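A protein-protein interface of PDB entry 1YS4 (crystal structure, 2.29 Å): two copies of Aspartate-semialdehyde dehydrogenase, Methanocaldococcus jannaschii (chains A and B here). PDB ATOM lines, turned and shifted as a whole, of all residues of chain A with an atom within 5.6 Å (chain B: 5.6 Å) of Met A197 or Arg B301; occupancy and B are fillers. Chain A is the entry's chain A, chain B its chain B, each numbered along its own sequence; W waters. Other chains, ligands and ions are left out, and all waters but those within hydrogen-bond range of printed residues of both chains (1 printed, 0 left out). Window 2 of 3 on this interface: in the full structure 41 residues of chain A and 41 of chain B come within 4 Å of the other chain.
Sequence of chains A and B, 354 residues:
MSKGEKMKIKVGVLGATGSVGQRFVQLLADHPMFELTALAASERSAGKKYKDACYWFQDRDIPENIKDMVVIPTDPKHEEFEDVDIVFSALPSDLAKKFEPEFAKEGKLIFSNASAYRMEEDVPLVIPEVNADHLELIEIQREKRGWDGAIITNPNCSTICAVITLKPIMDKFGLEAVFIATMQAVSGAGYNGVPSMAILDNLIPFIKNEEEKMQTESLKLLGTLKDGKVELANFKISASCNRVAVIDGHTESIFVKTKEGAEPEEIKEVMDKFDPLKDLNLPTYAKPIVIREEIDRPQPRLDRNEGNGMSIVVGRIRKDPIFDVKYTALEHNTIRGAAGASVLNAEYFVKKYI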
ATOM      1  N   PRO A 195     -20.516  29.441   6.428  1.00  0.00           N
ATOM      2  CA  PRO A 195     -19.523  28.442   6.030  1.00  0.00           C
ATOM      3  C   PRO A 195     -19.402  28.347   4.512  1.00  0.00           C
ATOM      4  O   PRO A 195     -20.375  28.599   3.798  1.00  0.00           O
ATOM      5  CB  PRO A 195     -20.076  27.140   6.614  1.00  0.00           C
ATOM      6  CG  PRO A 195     -21.531  27.376   6.810  1.00  0.00           C
ATOM      7  CD  PRO A 195     -21.697  28.835   7.075  1.00  0.00           C
ATOM      8  N   SER A 196     -18.214  27.989   4.030  1.00  0.00           N
ATOM      9  CA  SER A 196     -17.944  27.923   2.590  1.00  0.00           C
ATOM     10  C   SER A 196     -18.927  27.033   1.833  1.00  0.00           C
ATOM     11  O   SER A 196     -19.315  27.345   0.713  1.00  0.00           O
ATOM     12  CB  SER A 196     -16.502  27.489   2.321  1.00  0.00           C
ATOM     13  OG  SER A 196     -16.215  26.246   2.929  1.00  0.00           O
ATOM     14  N   MET A 197     -19.351  25.945   2.461  1.00  0.00           N
ATOM     15  CA  MET A 197     -20.265  25.003   1.819  1.00  0.00           C
ATOM     16  C   MET A 197     -21.732  25.421   1.797  1.00  0.00           C
ATOM     17  O   MET A 197     -22.562  24.755   1.183  1.00  0.00           O
ATOM     18  CB  MET A 197     -20.088  23.613   2.409  1.00  0.00           C
ATOM     19  CG  MET A 197     -18.793  22.997   1.937  1.00  0.00           C
ATOM     20  SD  MET A 197     -18.630  21.173   2.441  1.00  0.00           S
ATOM     21  CE  MET A 197     -20.086  20.434   1.393  1.00  0.00           C
ATOM     22  N   ALA A 198     -22.045  26.529   2.457  1.00  0.00           N
ATOM     23  CA  ALA A 198     -23.365  27.122   2.352  1.00  0.00           C
ATOM     24  C   ALA A 198     -23.529  27.844   1.013  1.00  0.00           C
ATOM     25  O   ALA A 198     -24.632  27.887   0.465  1.00  0.00           O
ATOM     26  CB  ALA A 198     -23.607  28.080   3.506  1.00  0.00           C
ATOM     27  N   ILE A 199     -22.433  28.397   0.488  1.00  0.00           N
ATOM     28  CA  ILE A 199     -22.498  29.232  -0.720  1.00  0.00           C
ATOM     29  C   ILE A 199     -21.601  28.799  -1.893  1.00  0.00           C
ATOM     30  O   ILE A 199     -21.638  29.409  -2.963  1.00  0.00           O
ATOM     31  CB  ILE A 199     -22.291  30.752  -0.398  1.00  0.00           C
ATOM     32  CG1 ILE A 199     -21.042  30.987   0.463  1.00  0.00           C
ATOM     33  CG2 ILE A 199     -23.536  31.327   0.280  1.00  0.00           C
ATOM     34  CD1 ILE A 199     -19.723  30.942  -0.299  1.00  0.00           C
ATOM     35  N   LEU A 200     -20.799  27.758  -1.698  1.00  0.00           N
ATOM     36  CA  LEU A 200     -19.973  27.235  -2.782  1.00  0.00           C
ATOM     37  C   LEU A 200     -20.840  26.356  -3.678  1.00  0.00           C
ATOM     38  O   LEU A 200     -21.330  25.316  -3.238  1.00  0.00           O
ATOM     39  CB  LEU A 200     -18.785  26.455  -2.216  1.00  0.00           C
ATOM     40  CG  LEU A 200     -17.434  26.479  -2.934  1.00  0.00           C
ATOM     41  CD1 LEU A 200     -17.049  27.883  -3.399  1.00  0.00           C
ATOM     42  CD2 LEU A 200     -16.365  25.908  -2.011  1.00  0.00           C
ATOM     43  N   ASP A 201     -21.042  26.792  -4.924  1.00  0.00           N
ATOM     44  CA  ASP A 201     -21.991  26.151  -5.855  1.00  0.00           C
ATOM     45  C   ASP A 201     -23.337  25.925  -5.161  1.00  0.00           C
ATOM     46  O   ASP A 201     -23.933  24.850  -5.252  1.00  0.00           O
ATOM     47  CB  ASP A 201     -21.415  24.838  -6.419  1.00  0.00           C
ATOM     48  CG  ASP A 201     -22.421  24.054  -7.272  1.00  0.00           C
ATOM     49  OD1 ASP A 201     -23.233  24.666  -8.005  1.00  0.00           O
ATOM     50  OD2 ASP A 201     -22.390  22.808  -7.214  1.00  0.00           O
ATOM     51  N   ASN A 202     -23.803  26.953  -4.459  1.00  0.00           N
ATOM     52  CA  ASN A 202     -24.975  26.839  -3.605  1.00  0.00           C
ATOM     53  C   ASN A 202     -25.475  28.213  -3.182  1.00  0.00           C
ATOM     54  O   ASN A 202     -24.779  29.217  -3.341  1.00  0.00           O
ATOM     55  CB  ASN A 202     -24.638  25.998  -2.360  1.00  0.00           C
ATOM     56  CG  ASN A 202     -25.874  25.448  -1.658  1.00  0.00           C
ATOM     57  OD1 ASN A 202     -26.824  24.994  -2.297  1.00  0.00           O
ATOM     58  ND2 ASN A 202     -25.856  25.475  -0.333  1.00  0.00           N
ATOM     59  N   ASP B 248     -25.389  24.291 -11.236  1.00  0.00           N
ATOM     60  CA  ASP B 248     -26.686  23.772 -11.660  1.00  0.00           C
ATOM     61  C   ASP B 248     -27.731  24.127 -10.607  1.00  0.00           C
ATOM     62  O   ASP B 248     -27.437  24.106  -9.410  1.00  0.00           O
ATOM     63  CB  ASP B 248     -26.636  22.248 -11.811  1.00  0.00           C
ATOM     64  CG  ASP B 248     -25.837  21.792 -13.024  1.00  0.00           C
ATOM     65  OD1 ASP B 248     -25.915  22.444 -14.086  1.00  0.00           O
ATOM     66  OD2 ASP B 248     -25.140  20.758 -12.920  1.00  0.00           O
ATOM     67  N   GLN B 299     -32.033  24.057  -1.291  1.00  0.00           N
ATOM     68  CA  GLN B 299     -30.733  24.595  -1.674  1.00  0.00           C
ATOM     69  C   GLN B 299     -30.288  23.877  -2.945  1.00  0.00           C
ATOM     70  O   GLN B 299     -30.423  22.655  -3.033  1.00  0.00           O
ATOM     71  CB  GLN B 299     -29.709  24.385  -0.557  1.00  0.00           C
ATOM     72  CG  GLN B 299     -30.001  25.180   0.704  1.00  0.00           C
ATOM     73  CD  GLN B 299     -29.064  24.844   1.847  1.00  0.00           C
ATOM     74  OE1 GLN B 299     -27.897  24.507   1.639  1.00  0.00           O
ATOM     75  NE2 GLN B 299     -29.570  24.942   3.067  1.00  0.00           N
ATOM     76  N   PRO B 300     -29.770  24.629  -3.937  1.00  0.00           N
ATOM     77  CA  PRO B 300     -29.380  24.018  -5.214  1.00  0.00           C
ATOM     78  C   PRO B 300     -28.525  22.760  -5.052  1.00  0.00           C
ATOM     79  O   PRO B 300     -28.879  21.716  -5.588  1.00  0.00           O
ATOM     80  CB  PRO B 300     -28.591  25.129  -5.917  1.00  0.00           C
ATOM     81  CG  PRO B 300     -29.138  26.385  -5.351  1.00  0.00           C
ATOM     82  CD  PRO B 300     -29.528  26.084  -3.927  1.00  0.00           C
ATOM     83  N   ARG B 301     -27.436  22.843  -4.295  1.00  0.00           N
ATOM     84  CA  ARG B 301     -26.538  21.699  -4.173  1.00  0.00           C
ATOM     85  C   ARG B 301     -27.158  20.492  -3.473  1.00  0.00           C
ATOM     86  O   ARG B 301     -26.874  19.356  -3.840  1.00  0.00           O
ATOM     87  CB  ARG B 301     -25.220  22.082  -3.508  1.00  0.00           C
ATOM     88  CG  ARG B 301     -24.026  21.536  -4.270  1.00  0.00           C
ATOM     89  CD  ARG B 301     -22.745  21.650  -3.494  1.00  0.00           C
ATOM     90  NE  ARG B 301     -22.389  20.377  -2.875  1.00  0.00           N
ATOM     91  CZ  ARG B 301     -22.401  20.141  -1.566  1.00  0.00           C
ATOM     92  NH1 ARG B 301     -22.743  21.099  -0.709  1.00  0.00           N
ATOM     93  NH2 ARG B 301     -22.058  18.939  -1.118  1.00  0.00           N
ATOM     94  N   LEU B 302     -28.009  20.743  -2.481  1.00  0.00           N
ATOM     95  CA  LEU B 302     -28.619  19.666  -1.704  1.00  0.00           C
ATOM     96  C   LEU B 302     -29.823  19.027  -2.388  1.00  0.00           C
ATOM     97  O   LEU B 302     -30.113  17.854  -2.156  1.00  0.00           O
ATOM     98  CB  LEU B 302     -29.040  20.163  -0.314  1.00  0.00           C
ATOM     99  CG  LEU B 302     -28.030  20.877   0.588  1.00  0.00           C
ATOM    100  CD1 LEU B 302     -28.596  21.042   1.988  1.00  0.00           C
ATOM    101  CD2 LEU B 302     -26.704  20.134   0.632  1.00  0.00           C
ATOM    102  N   ASP B 303     -30.520  19.795  -3.225  1.00  0.00           N
ATOM    103  CA  ASP B 303     -31.847  19.386  -3.688  1.00  0.00           C
ATOM    104  C   ASP B 303     -32.049  19.218  -5.198  1.00  0.00           C
ATOM    105  O   ASP B 303     -33.085  18.707  -5.620  1.00  0.00           O
ATOM    106  CB  ASP B 303     -32.910  20.336  -3.119  1.00  0.00           C
ATOM    107  CG  ASP B 303     -33.031  20.240  -1.613  1.00  0.00           C
ATOM    108  OD1 ASP B 303     -33.274  19.129  -1.103  1.00  0.00           O
ATOM    109  OD2 ASP B 303     -32.888  21.277  -0.936  1.00  0.00           O
ATOM    110  N   ARG B 304     -31.076  19.628  -6.008  1.00  0.00           N
ATOM    111  CA  ARG B 304     -31.250  19.596  -7.470  1.00  0.00           C
ATOM    112  C   ARG B 304     -31.304  18.181  -8.067  1.00  0.00           C
ATOM    113  O   ARG B 304     -31.826  17.998  -9.168  1.00  0.00           O
ATOM    114  CB  ARG B 304     -30.200  20.460  -8.187  1.00  0.00           C
ATOM    115  CG  ARG B 304     -28.792  19.888  -8.187  1.00  0.00           C
ATOM    116  CD  ARG B 304     -27.777  20.961  -8.531  1.00  0.00           C
ATOM    117  NE  ARG B 304     -26.406  20.518  -8.298  1.00  0.00           N
ATOM    118  CZ  ARG B 304     -25.389  21.330  -8.026  1.00  0.00           C
ATOM    119  NH1 ARG B 304     -24.181  20.824  -7.827  1.00  0.00           N
ATOM    120  NH2 ARG B 304     -25.574  22.645  -7.937  1.00  0.00           N
HETATM  121  O   HOH W   1     -21.948  23.590  -1.061  1.00  0.00           O
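Of chain A, only Met A197, Leu A200, Asp A201 and Asn A202 come within 4 Å of Arg B301.
Printed residues of chain B within 4 Å of Asp A201: Asp B248, Arg B301 and Arg B304.
Of the printed residues of chain A, Gln B299 touches Asn A202 (3.0 Å).
The nearest printed residue of chain A that does not touch Arg B301 is Ala A198 (6.3 Å).
The nearest printed residue of chain A that does not touch Asp B248 is Asn A202 (6.8 Å).
O of Asp B248 lies within hydrogen-bond range of NH2 of Arg B304.
The backbone carbonyl oxygen of Ala A198 is in hydrogen-bond range of the side-chain amide nitrogen of Asn A202 (2.8 Å).
The backbone NH (N) of Gln B299 sits at hydrogen-bond distance from the side-chain carboxylate (OD2) of Asp B303.
OD2 of Asp A201 is in salt-bridge range of NH1 of Arg B304, 2.7 Å away.
The side-chain amide oxygen (OD1) of Asn A202 lies close to the backbone nitrogen (N) of Pro B300, 3.4 Å away.
N of Arg B301 sits at hydrogen-bond distance from OD1 of Asn A202, 3.0 Å away.
OE1 of Gln B299 lies within hydrogen-bond range of ND2 of Asn A202.
No position is printed for both chains.
Of the 8 pairs that touch across the chains among the printed residues, none has its exchanged pair printed and touching as well.
Water W1 lies within hydrogen-bond range of O of Met A197 (2.6 Å), NH1 of Arg B301 (2.6 Å) and O of Leu A200 (2.8 Å).
Among the printed residues, pairs that only touch across the chains: Met A197 with Arg B301 (3.5 Å), Leu A200 with Arg B301 (3.9 Å), Asp A201 with Asp B248 (3.9 Å) and Asp A201 with Arg B301 (3.5 Å).
Of the 8 printed residues of chain A, 4 touch a printed residue of chain B.
Hydrophobic or aromatic side chains of chain A that line the printed part of chain B: Met A197.
Of the 7 printed residues of chain B, 5 touch a printed residue of chain A.
Printed residues of chain B that touch a printed residue of chain A: Asp B248, Gln B299, Pro B300, Arg B301 and Arg B304.
Hydrophobic or aromatic side chains of chain B within 4 Å of the printed part of chain A: Pro B300.
Among the printed residues, 8 pairs touch across the chains.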
